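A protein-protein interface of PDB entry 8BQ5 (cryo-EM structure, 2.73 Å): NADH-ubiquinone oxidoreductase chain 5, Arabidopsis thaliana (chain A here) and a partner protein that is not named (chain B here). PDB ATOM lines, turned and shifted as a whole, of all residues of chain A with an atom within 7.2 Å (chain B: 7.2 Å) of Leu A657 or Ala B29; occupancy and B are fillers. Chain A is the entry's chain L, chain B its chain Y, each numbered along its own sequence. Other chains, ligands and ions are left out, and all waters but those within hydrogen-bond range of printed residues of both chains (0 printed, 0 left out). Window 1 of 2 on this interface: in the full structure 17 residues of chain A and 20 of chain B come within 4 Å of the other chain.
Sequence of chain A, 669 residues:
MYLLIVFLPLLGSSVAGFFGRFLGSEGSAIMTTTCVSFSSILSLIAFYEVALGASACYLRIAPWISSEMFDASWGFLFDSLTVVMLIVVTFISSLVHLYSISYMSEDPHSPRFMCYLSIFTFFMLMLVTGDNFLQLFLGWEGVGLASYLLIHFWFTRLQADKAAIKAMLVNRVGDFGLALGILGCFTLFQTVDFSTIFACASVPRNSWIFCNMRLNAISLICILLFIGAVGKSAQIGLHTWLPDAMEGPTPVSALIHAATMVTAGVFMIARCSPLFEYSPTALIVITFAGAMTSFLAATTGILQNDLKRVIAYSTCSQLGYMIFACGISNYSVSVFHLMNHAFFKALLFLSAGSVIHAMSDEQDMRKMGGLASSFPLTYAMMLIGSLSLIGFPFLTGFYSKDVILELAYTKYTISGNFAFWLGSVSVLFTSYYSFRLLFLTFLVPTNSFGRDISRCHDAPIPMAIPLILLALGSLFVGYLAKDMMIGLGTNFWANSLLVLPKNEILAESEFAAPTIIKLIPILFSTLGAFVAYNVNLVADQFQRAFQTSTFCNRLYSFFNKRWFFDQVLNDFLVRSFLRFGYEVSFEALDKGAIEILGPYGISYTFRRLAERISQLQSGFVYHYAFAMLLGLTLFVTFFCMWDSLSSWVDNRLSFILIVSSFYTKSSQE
Hydrophobic or aromatic side chains of chain B within 4 Å of the printed part of chain A: Ala B29, Tyr B33, Phe B69 and Ile B72. Printed residues of chain A that touch a printed residue of chain B: Leu A653, Ile A656, Leu A657, Val A659, Ser A660 and Ser A661. Hydrophobic or aromatic side chains of chain A that line the printed part of chain B: Leu A653, Ile A656, Leu A657 and Val A659. Along chain A the printed residues that touch a printed residue of chain B span positions 653 to 661. Among the printed residues, 12 pairs touch across the chains. Among the printed residues, no Asp or Glu carboxylate lies within 4 Å of a Lys or Arg side-chain nitrogen of the other chain.
Leu A653 touches Gly B22. O of Gly B73 touches CD2 of Leu A653, 3.96 Å away. CG2 of Thr B127 touches CD1 of Ile A656, at 3.6 Å. CA of Gly B26 touches CD1 of Leu A657, at 3.8 Å. CB of Ala B29 touches CD1 of Leu A657, 3.8 Å away. Phe B69 touches Leu A657 (CG to CD2, 3.4 Å). Ile B72 touches Leu A657 (CG2 to CD2, 3.6 Å). OG of Ser A660 touches CG1 of Ile B72, 3.8 Å away. O of Ser A661 touches OH of Tyr B33, 3.6 Å away. CZ of Phe B69 touches OG of Ser A661, at 3.4 Å.
Of chain B, only Gly B26 (3.8 Å), Ala B29 (3.8 Å), Phe B69 (3.4 Å) and Ile B72 (3.6 Å) come within 4 Å of Leu A657. Ala B29 touches just one residue of chain A: Leu A657. No residue of chain A comes within 4 Å of Gly B28. Of the printed residues of chain A, Thr B127 touches Ile A656 and Val A659. Printed residues of chain A within 4 Å of Ile B72: Ile A656 (3.7 Å), Leu A657 (3.6 Å) and Ser A660 (3.8 Å). Of the printed residues of chain A, Gly B26 touches Leu A657 (3.8 Å). Of the printed residues of chain A, Gly B22 touches Leu A653 (3.7 Å).
The backbone carbonyl oxygen (O) of Leu A657 is in hydrogen-bond range of the side-chain hydroxyl (OG) of Ser A661 (2.6 Å). The backbone carbonyl oxygen (O) of Ile A658 sits at hydrogen-bond distance from the side-chain hydroxyl (OG) of Ser A661, at 3.1 Å.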
ATOM      1  N   ARG A 652      25.004  21.577   1.839  1.00  0.00           N
ATOM      2  CA  ARG A 652      25.912  22.476   1.138  1.00  0.00           C
ATOM      3  C   ARG A 652      26.218  21.958  -0.261  1.00  0.00           C
ATOM      4  O   ARG A 652      26.069  22.679  -1.254  1.00  0.00           O
ATOM      5  CB  ARG A 652      27.197  22.618   1.950  1.00  0.00           C
ATOM      6  CG  ARG A 652      27.014  22.240   3.407  1.00  0.00           C
ATOM      7  CD  ARG A 652      28.195  22.662   4.243  1.00  0.00           C
ATOM      8  NE  ARG A 652      28.589  24.036   3.968  1.00  0.00           N
ATOM      9  CZ  ARG A 652      29.680  24.607   4.459  1.00  0.00           C
ATOM     10  NH1 ARG A 652      30.499  23.952   5.262  1.00  0.00           N
ATOM     11  NH2 ARG A 652      29.949  25.870   4.141  1.00  0.00           N
ATOM     12  N   LEU A 653      26.633  20.693  -0.356  1.00  0.00           N
ATOM     13  CA  LEU A 653      27.063  20.140  -1.637  1.00  0.00           C
ATOM     14  C   LEU A 653      25.889  19.987  -2.593  1.00  0.00           C
ATOM     15  O   LEU A 653      26.064  20.017  -3.817  1.00  0.00           O
ATOM     16  CB  LEU A 653      27.753  18.789  -1.432  1.00  0.00           C
ATOM     17  CG  LEU A 653      29.070  18.813  -0.652  1.00  0.00           C
ATOM     18  CD1 LEU A 653      29.566  17.398  -0.397  1.00  0.00           C
ATOM     19  CD2 LEU A 653      30.119  19.629  -1.391  1.00  0.00           C
ATOM     20  N   SER A 654      24.681  19.809  -2.054  1.00  0.00           N
ATOM     21  CA  SER A 654      23.510  19.689  -2.907  1.00  0.00           C
ATOM     22  C   SER A 654      23.341  20.937  -3.762  1.00  0.00           C
ATOM     23  O   SER A 654      23.349  20.860  -4.994  1.00  0.00           O
ATOM     24  CB  SER A 654      22.261  19.432  -2.054  1.00  0.00           C
ATOM     25  OG  SER A 654      22.010  18.041  -1.928  1.00  0.00           O
ATOM     26  N   PHE A 655      23.278  22.108  -3.122  1.00  0.00           N
ATOM     27  CA  PHE A 655      23.026  23.341  -3.862  1.00  0.00           C
ATOM     28  C   PHE A 655      24.268  23.799  -4.615  1.00  0.00           C
ATOM     29  O   PHE A 655      24.167  24.554  -5.587  1.00  0.00           O
ATOM     30  CB  PHE A 655      22.525  24.432  -2.917  1.00  0.00           C
ATOM     31  CG  PHE A 655      21.091  24.254  -2.494  1.00  0.00           C
ATOM     32  CD1 PHE A 655      20.163  25.254  -2.709  1.00  0.00           C
ATOM     33  CD2 PHE A 655      20.676  23.089  -1.872  1.00  0.00           C
ATOM     34  CE1 PHE A 655      18.848  25.096  -2.318  1.00  0.00           C
ATOM     35  CE2 PHE A 655      19.363  22.923  -1.480  1.00  0.00           C
ATOM     36  CZ  PHE A 655      18.446  23.927  -1.704  1.00  0.00           C
ATOM     37  N   ILE A 656      25.446  23.350  -4.178  1.00  0.00           N
ATOM     38  CA  ILE A 656      26.681  23.621  -4.909  1.00  0.00           C
ATOM     39  C   ILE A 656      26.617  23.003  -6.299  1.00  0.00           C
ATOM     40  O   ILE A 656      26.970  23.633  -7.306  1.00  0.00           O
ATOM     41  CB  ILE A 656      27.887  23.085  -4.115  1.00  0.00           C
ATOM     42  CG1 ILE A 656      28.263  24.034  -2.972  1.00  0.00           C
ATOM     43  CG2 ILE A 656      29.069  22.818  -5.037  1.00  0.00           C
ATOM     44  CD1 ILE A 656      29.129  25.186  -3.377  1.00  0.00           C
ATOM     45  N   LEU A 657      26.160  21.753  -6.373  1.00  0.00           N
ATOM     46  CA  LEU A 657      26.150  21.047  -7.647  1.00  0.00           C
ATOM     47  C   LEU A 657      25.079  21.602  -8.578  1.00  0.00           C
ATOM     48  O   LEU A 657      25.285  21.669  -9.797  1.00  0.00           O
ATOM     49  CB  LEU A 657      25.953  19.552  -7.407  1.00  0.00           C
ATOM     50  CG  LEU A 657      27.242  18.826  -7.011  1.00  0.00           C
ATOM     51  CD1 LEU A 657      26.966  17.397  -6.568  1.00  0.00           C
ATOM     52  CD2 LEU A 657      28.256  18.862  -8.142  1.00  0.00           C
ATOM     53  N   ILE A 658      23.933  22.016  -8.027  1.00  0.00           N
ATOM     54  CA  ILE A 658      22.877  22.578  -8.867  1.00  0.00           C
ATOM     55  C   ILE A 658      23.360  23.844  -9.564  1.00  0.00           C
ATOM     56  O   ILE A 658      23.196  24.002 -10.779  1.00  0.00           O
ATOM     57  CB  ILE A 658      21.590  22.838  -8.060  1.00  0.00           C
ATOM     58  CG1 ILE A 658      21.074  21.561  -7.393  1.00  0.00           C
ATOM     59  CG2 ILE A 658      20.518  23.459  -8.940  1.00  0.00           C
ATOM     60  CD1 ILE A 658      20.765  21.702  -5.933  1.00  0.00           C
ATOM     61  N   VAL A 659      23.962  24.768  -8.811  1.00  0.00           N
ATOM     62  CA  VAL A 659      24.453  25.989  -9.442  1.00  0.00           C
ATOM     63  C   VAL A 659      25.602  25.667 -10.388  1.00  0.00           C
ATOM     64  O   VAL A 659      25.705  26.243 -11.479  1.00  0.00           O
ATOM     65  CB  VAL A 659      24.855  27.040  -8.388  1.00  0.00           C
ATOM     66  CG1 VAL A 659      23.620  27.620  -7.714  1.00  0.00           C
ATOM     67  CG2 VAL A 659      25.800  26.458  -7.364  1.00  0.00           C
ATOM     68  N   SER A 660      26.469  24.725 -10.001  1.00  0.00           N
ATOM     69  CA  SER A 660      27.577  24.350 -10.873  1.00  0.00           C
ATOM     70  C   SER A 660      27.091  23.733 -12.179  1.00  0.00           C
ATOM     71  O   SER A 660      27.828  23.727 -13.172  1.00  0.00           O
ATOM     72  CB  SER A 660      28.514  23.384 -10.147  1.00  0.00           C
ATOM     73  OG  SER A 660      29.574  22.971 -10.992  1.00  0.00           O
ATOM     74  N   SER A 661      25.861  23.210 -12.201  1.00  0.00           N
ATOM     75  CA  SER A 661      25.329  22.625 -13.430  1.00  0.00           C
ATOM     76  C   SER A 661      25.202  23.654 -14.544  1.00  0.00           C
ATOM     77  O   SER A 661      25.346  23.311 -15.723  1.00  0.00           O
ATOM     78  CB  SER A 661      23.967  21.979 -13.169  1.00  0.00           C
ATOM     79  OG  SER A 661      23.955  21.259 -11.951  1.00  0.00           O
ATOM     80  N   PHE A 662      24.936  24.917 -14.196  1.00  0.00           N
ATOM     81  CA  PHE A 662      24.669  25.926 -15.216  1.00  0.00           C
ATOM     82  C   PHE A 662      25.871  26.141 -16.126  1.00  0.00           C
ATOM     83  O   PHE A 662      25.713  26.597 -17.265  1.00  0.00           O
ATOM     84  CB  PHE A 662      24.266  27.248 -14.560  1.00  0.00           C
ATOM     85  CG  PHE A 662      23.029  27.159 -13.710  1.00  0.00           C
ATOM     86  CD1 PHE A 662      22.124  26.121 -13.868  1.00  0.00           C
ATOM     87  CD2 PHE A 662      22.772  28.121 -12.747  1.00  0.00           C
ATOM     88  CE1 PHE A 662      20.992  26.044 -13.080  1.00  0.00           C
ATOM     89  CE2 PHE A 662      21.641  28.050 -11.959  1.00  0.00           C
ATOM     90  CZ  PHE A 662      20.750  27.010 -12.125  1.00  0.00           C
ATOM     91  N   GLY B  22      31.822  13.252   0.011  1.00  0.00           N
ATOM     92  CA  GLY B  22      31.457  14.313  -0.910  1.00  0.00           C
ATOM     93  C   GLY B  22      31.752  13.955  -2.352  1.00  0.00           C
ATOM     94  O   GLY B  22      30.937  14.206  -3.243  1.00  0.00           O
ATOM     95  N   SER B  23      32.919  13.354  -2.604  1.00  0.00           N
ATOM     96  CA  SER B  23      33.236  12.912  -3.958  1.00  0.00           C
ATOM     97  C   SER B  23      32.246  11.859  -4.439  1.00  0.00           C
ATOM     98  O   SER B  23      31.809  11.890  -5.595  1.00  0.00           O
ATOM     99  CB  SER B  23      34.664  12.369  -4.022  1.00  0.00           C
ATOM    100  OG  SER B  23      35.545  13.130  -3.215  1.00  0.00           O
ATOM    101  N   ILE B  24      31.879  10.919  -3.566  1.00  0.00           N
ATOM    102  CA  ILE B  24      30.946   9.861  -3.956  1.00  0.00           C
ATOM    103  C   ILE B  24      29.576  10.447  -4.286  1.00  0.00           C
ATOM    104  O   ILE B  24      28.951  10.089  -5.297  1.00  0.00           O
ATOM    105  CB  ILE B  24      30.853   8.801  -2.845  1.00  0.00           C
ATOM    106  CG1 ILE B  24      32.204   8.112  -2.655  1.00  0.00           C
ATOM    107  CG2 ILE B  24      29.774   7.781  -3.170  1.00  0.00           C
ATOM    108  CD1 ILE B  24      32.199   7.047  -1.585  1.00  0.00           C
ATOM    109  N   THR B  25      29.087  11.352  -3.435  1.00  0.00           N
ATOM    110  CA  THR B  25      27.801  11.996  -3.680  1.00  0.00           C
ATOM    111  C   THR B  25      27.826  12.797  -4.975  1.00  0.00           C
ATOM    112  O   THR B  25      26.867  12.763  -5.757  1.00  0.00           O
ATOM    113  CB  THR B  25      27.436  12.893  -2.497  1.00  0.00           C
ATOM    114  OG1 THR B  25      27.131  12.081  -1.356  1.00  0.00           O
ATOM    115  CG2 THR B  25      26.239  13.772  -2.828  1.00  0.00           C
ATOM    116  N   GLY B  26      28.918  13.523  -5.217  1.00  0.00           N
ATOM    117  CA  GLY B  26      29.041  14.262  -6.458  1.00  0.00           C
ATOM    118  C   GLY B  26      29.055  13.358  -7.673  1.00  0.00           C
ATOM    119  O   GLY B  26      28.461  13.682  -8.701  1.00  0.00           O
ATOM    120  N   PHE B  27      29.731  12.213  -7.577  1.00  0.00           N
ATOM    121  CA  PHE B  27      29.734  11.283  -8.700  1.00  0.00           C
ATOM    122  C   PHE B  27      28.337  10.745  -8.974  1.00  0.00           C
ATOM    123  O   PHE B  27      27.928  10.623 -10.136  1.00  0.00           O
ATOM    124  CB  PHE B  27      30.704  10.133  -8.446  1.00  0.00           C
ATOM    125  CG  PHE B  27      30.789   9.167  -9.587  1.00  0.00           C
ATOM    126  CD1 PHE B  27      31.581   9.447 -10.684  1.00  0.00           C
ATOM    127  CD2 PHE B  27      30.069   7.986  -9.567  1.00  0.00           C
ATOM    128  CE1 PHE B  27      31.657   8.566 -11.740  1.00  0.00           C
ATOM    129  CE2 PHE B  27      30.142   7.102 -10.621  1.00  0.00           C
ATOM    130  CZ  PHE B  27      30.938   7.392 -11.709  1.00  0.00           C
ATOM    131  N   GLY B  28      27.589  10.415  -7.920  1.00  0.00           N
ATOM    132  CA  GLY B  28      26.218   9.969  -8.122  1.00  0.00           C
ATOM    133  C   GLY B  28      25.357  11.030  -8.783  1.00  0.00           C
ATOM    134  O   GLY B  28      24.617  10.754  -9.739  1.00  0.00           O
ATOM    135  N   ALA B  29      25.454  12.267  -8.288  1.00  0.00           N
ATOM    136  CA  ALA B  29      24.681  13.361  -8.863  1.00  0.00           C
ATOM    137  C   ALA B  29      25.067  13.605 -10.316  1.00  0.00           C
ATOM    138  O   ALA B  29      24.202  13.854 -11.161  1.00  0.00           O
ATOM    139  CB  ALA B  29      24.873  14.631  -8.036  1.00  0.00           C
ATOM    140  N   GLY B  30      26.362  13.538 -10.623  1.00  0.00           N
ATOM    141  CA  GLY B  30      26.800  13.731 -11.994  1.00  0.00           C
ATOM    142  C   GLY B  30      26.327  12.626 -12.915  1.00  0.00           C
ATOM    143  O   GLY B  30      25.977  12.880 -14.068  1.00  0.00           O
ATOM    144  N   THR B  31      26.302  11.388 -12.421  1.00  0.00           N
ATOM    145  CA  THR B  31      25.772  10.287 -13.216  1.00  0.00           C
ATOM    146  C   THR B  31      24.302  10.508 -13.545  1.00  0.00           C
ATOM    147  O   THR B  31      23.885  10.377 -14.703  1.00  0.00           O
ATOM    148  CB  THR B  31      25.966   8.966 -12.473  1.00  0.00           C
ATOM    149  OG1 THR B  31      27.363   8.654 -12.408  1.00  0.00           O
ATOM    150  CG2 THR B  31      25.231   7.841 -13.185  1.00  0.00           C
ATOM    151  N   ILE B  32      23.501  10.869 -12.538  1.00  0.00           N
ATOM    152  CA  ILE B  32      22.074  11.088 -12.777  1.00  0.00           C
ATOM    153  C   ILE B  32      21.853  12.271 -13.717  1.00  0.00           C
ATOM    154  O   ILE B  32      21.023  12.213 -14.638  1.00  0.00           O
ATOM    155  CB  ILE B  32      21.332  11.275 -11.442  1.00  0.00           C
ATOM    156  CG1 ILE B  32      21.550  10.058 -10.541  1.00  0.00           C
ATOM    157  CG2 ILE B  32      19.851  11.507 -11.679  1.00  0.00           C
ATOM    158  CD1 ILE B  32      21.474  10.365  -9.065  1.00  0.00           C
ATOM    159  N   TYR B  33      22.586  13.364 -13.498  1.00  0.00           N
ATOM    160  CA  TYR B  33      22.439  14.550 -14.334  1.00  0.00           C
ATOM    161  C   TYR B  33      22.847  14.265 -15.775  1.00  0.00           C
ATOM    162  O   TYR B  33      22.184  14.717 -16.716  1.00  0.00           O
ATOM    163  CB  TYR B  33      23.265  15.690 -13.737  1.00  0.00           C
ATOM    164  CG  TYR B  33      23.355  16.934 -14.583  1.00  0.00           C
ATOM    165  CD1 TYR B  33      22.221  17.657 -14.923  1.00  0.00           C
ATOM    166  CD2 TYR B  33      24.582  17.392 -15.035  1.00  0.00           C
ATOM    167  CE1 TYR B  33      22.312  18.803 -15.686  1.00  0.00           C
ATOM    168  CE2 TYR B  33      24.681  18.529 -15.803  1.00  0.00           C
ATOM    169  CZ  TYR B  33      23.546  19.227 -16.133  1.00  0.00           C
ATOM    170  OH  TYR B  33      23.657  20.362 -16.903  1.00  0.00           O
ATOM    171  N   GLY B  34      23.934  13.516 -15.970  1.00  0.00           N
ATOM    172  CA  GLY B  34      24.328  13.136 -17.314  1.00  0.00           C
ATOM    173  C   GLY B  34      23.316  12.224 -17.975  1.00  0.00           C
ATOM    174  O   GLY B  34      23.074  12.326 -19.179  1.00  0.00           O
ATOM    175  N   THR B  35      22.709  11.322 -17.200  1.00  0.00           N
ATOM    176  CA  THR B  35      21.639  10.486 -17.732  1.00  0.00           C
ATOM    177  C   THR B  35      20.490  11.340 -18.251  1.00  0.00           C
ATOM    178  O   THR B  35      19.995  11.134 -19.367  1.00  0.00           O
ATOM    179  CB  THR B  35      21.138   9.529 -16.651  1.00  0.00           C
ATOM    180  OG1 THR B  35      22.240   8.795 -16.104  1.00  0.00           O
ATOM    181  CG2 THR B  35      20.132   8.559 -17.231  1.00  0.00           C
ATOM    182  N   ILE B  36      20.057  12.313 -17.445  1.00  0.00           N
ATOM    183  CA  ILE B  36      18.951  13.184 -17.844  1.00  0.00           C
ATOM    184  C   ILE B  36      19.318  13.977 -19.093  1.00  0.00           C
ATOM    185  O   ILE B  36      18.527  14.083 -20.039  1.00  0.00           O
ATOM    186  CB  ILE B  36      18.552  14.111 -16.682  1.00  0.00           C
ATOM    187  CG1 ILE B  36      17.736  13.344 -15.643  1.00  0.00           C
ATOM    188  CG2 ILE B  36      17.774  15.316 -17.191  1.00  0.00           C
ATOM    189  CD1 ILE B  36      17.897  13.869 -14.244  1.00  0.00           C
ATOM    190  N   HIS B  65      29.968  13.454 -16.802  1.00  0.00           N
ATOM    191  CA  HIS B  65      29.340  14.351 -15.839  1.00  0.00           C
ATOM    192  C   HIS B  65      29.512  13.847 -14.413  1.00  0.00           C
ATOM    193  O   HIS B  65      29.640  14.649 -13.480  1.00  0.00           O
ATOM    194  CB  HIS B  65      27.868  14.546 -16.190  1.00  0.00           C
ATOM    195  CG  HIS B  65      27.628  15.703 -17.107  1.00  0.00           C
ATOM    196  ND1 HIS B  65      27.623  15.578 -18.480  1.00  0.00           N
ATOM    197  CD2 HIS B  65      27.399  17.012 -16.848  1.00  0.00           C
ATOM    198  CE1 HIS B  65      27.398  16.759 -19.026  1.00  0.00           C
ATOM    199  NE2 HIS B  65      27.254  17.645 -18.058  1.00  0.00           N
ATOM    200  N   GLY B  66      29.545  12.526 -14.222  1.00  0.00           N
ATOM    201  CA  GLY B  66      29.853  11.993 -12.908  1.00  0.00           C
ATOM    202  C   GLY B  66      31.250  12.361 -12.454  1.00  0.00           C
ATOM    203  O   GLY B  66      31.454  12.746 -11.302  1.00  0.00           O
ATOM    204  N   THR B  68      33.023  14.997 -13.461  1.00  0.00           N
ATOM    205  CA  THR B  68      33.068  16.434 -13.191  1.00  0.00           C
ATOM    206  C   THR B  68      32.401  16.780 -11.860  1.00  0.00           C
ATOM    207  O   THR B  68      32.957  17.543 -11.052  1.00  0.00           O
ATOM    208  CB  THR B  68      32.415  17.199 -14.343  1.00  0.00           C
ATOM    209  OG1 THR B  68      33.349  17.328 -15.423  1.00  0.00           O
ATOM    210  CG2 THR B  68      31.973  18.583 -13.900  1.00  0.00           C
ATOM    211  N   PHE B  69      31.221  16.216 -11.600  1.00  0.00           N
ATOM    212  CA  PHE B  69      30.523  16.543 -10.364  1.00  0.00           C
ATOM    213  C   PHE B  69      31.228  15.954  -9.149  1.00  0.00           C
ATOM    214  O   PHE B  69      31.229  16.574  -8.080  1.00  0.00           O
ATOM    215  CB  PHE B  69      29.075  16.064 -10.437  1.00  0.00           C
ATOM    216  CG  PHE B  69      28.142  17.056 -11.067  1.00  0.00           C
ATOM    217  CD1 PHE B  69      28.624  18.030 -11.924  1.00  0.00           C
ATOM    218  CD2 PHE B  69      26.784  17.016 -10.801  1.00  0.00           C
ATOM    219  CE1 PHE B  69      27.769  18.943 -12.507  1.00  0.00           C
ATOM    220  CE2 PHE B  69      25.923  17.927 -11.382  1.00  0.00           C
ATOM    221  CZ  PHE B  69      26.417  18.893 -12.233  1.00  0.00           C
ATOM    222  N   ALA B  70      31.839  14.774  -9.288  1.00  0.00           N
ATOM    223  CA  ALA B  70      32.646  14.233  -8.203  1.00  0.00           C
ATOM    224  C   ALA B  70      33.844  15.127  -7.920  1.00  0.00           C
ATOM    225  O   ALA B  70      34.213  15.331  -6.758  1.00  0.00           O
ATOM    226  CB  ALA B  70      33.103  12.816  -8.542  1.00  0.00           C
ATOM    227  N   ALA B  71      34.466  15.666  -8.971  1.00  0.00           N
ATOM    228  CA  ALA B  71      35.567  16.602  -8.775  1.00  0.00           C
ATOM    229  C   ALA B  71      35.112  17.817  -7.979  1.00  0.00           C
ATOM    230  O   ALA B  71      35.784  18.236  -7.026  1.00  0.00           O
ATOM    231  CB  ALA B  71      36.143  17.027 -10.126  1.00  0.00           C
ATOM    232  N   ILE B  72      33.964  18.393  -8.352  1.00  0.00           N
ATOM    233  CA  ILE B  72      33.447  19.539  -7.602  1.00  0.00           C
ATOM    234  C   ILE B  72      33.209  19.151  -6.147  1.00  0.00           C
ATOM    235  O   ILE B  72      33.679  19.820  -5.218  1.00  0.00           O
ATOM    236  CB  ILE B  72      32.159  20.091  -8.242  1.00  0.00           C
ATOM    237  CG1 ILE B  72      32.464  21.227  -9.214  1.00  0.00           C
ATOM    238  CG2 ILE B  72      31.214  20.630  -7.180  1.00  0.00           C
ATOM    239  CD1 ILE B  72      33.084  20.779 -10.485  1.00  0.00           C
ATOM    240  N   GLY B  73      32.492  18.043  -5.929  1.00  0.00           N
ATOM    241  CA  GLY B  73      32.089  17.661  -4.589  1.00  0.00           C
ATOM    242  C   GLY B  73      33.236  17.235  -3.704  1.00  0.00           C
ATOM    243  O   GLY B  73      33.102  17.263  -2.475  1.00  0.00           O
ATOM    244  N   LEU B 124      29.886  30.135  -7.043  1.00  0.00           N
ATOM    245  CA  LEU B 124      30.015  29.115  -6.009  1.00  0.00           C
ATOM    246  C   LEU B 124      30.284  29.741  -4.643  1.00  0.00           C
ATOM    247  O   LEU B 124      29.720  29.301  -3.632  1.00  0.00           O
ATOM    248  CB  LEU B 124      31.130  28.142  -6.398  1.00  0.00           C
ATOM    249  CG  LEU B 124      30.826  26.953  -7.330  1.00  0.00           C
ATOM    250  CD1 LEU B 124      30.451  27.422  -8.710  1.00  0.00           C
ATOM    251  CD2 LEU B 124      31.983  25.965  -7.430  1.00  0.00           C
ATOM    252  N   THR B 127      26.997  31.087  -3.409  1.00  0.00           N
ATOM    253  CA  THR B 127      26.072  30.038  -2.990  1.00  0.00           C
ATOM    254  C   THR B 127      26.524  29.396  -1.680  1.00  0.00           C
ATOM    255  O   THR B 127      25.708  28.844  -0.933  1.00  0.00           O
ATOM    256  CB  THR B 127      25.916  28.993  -4.101  1.00  0.00           C
ATOM    257  OG1 THR B 127      24.668  28.309  -3.941  1.00  0.00           O
ATOM    258  CG2 THR B 127      27.034  27.975  -4.062  1.00  0.00           C
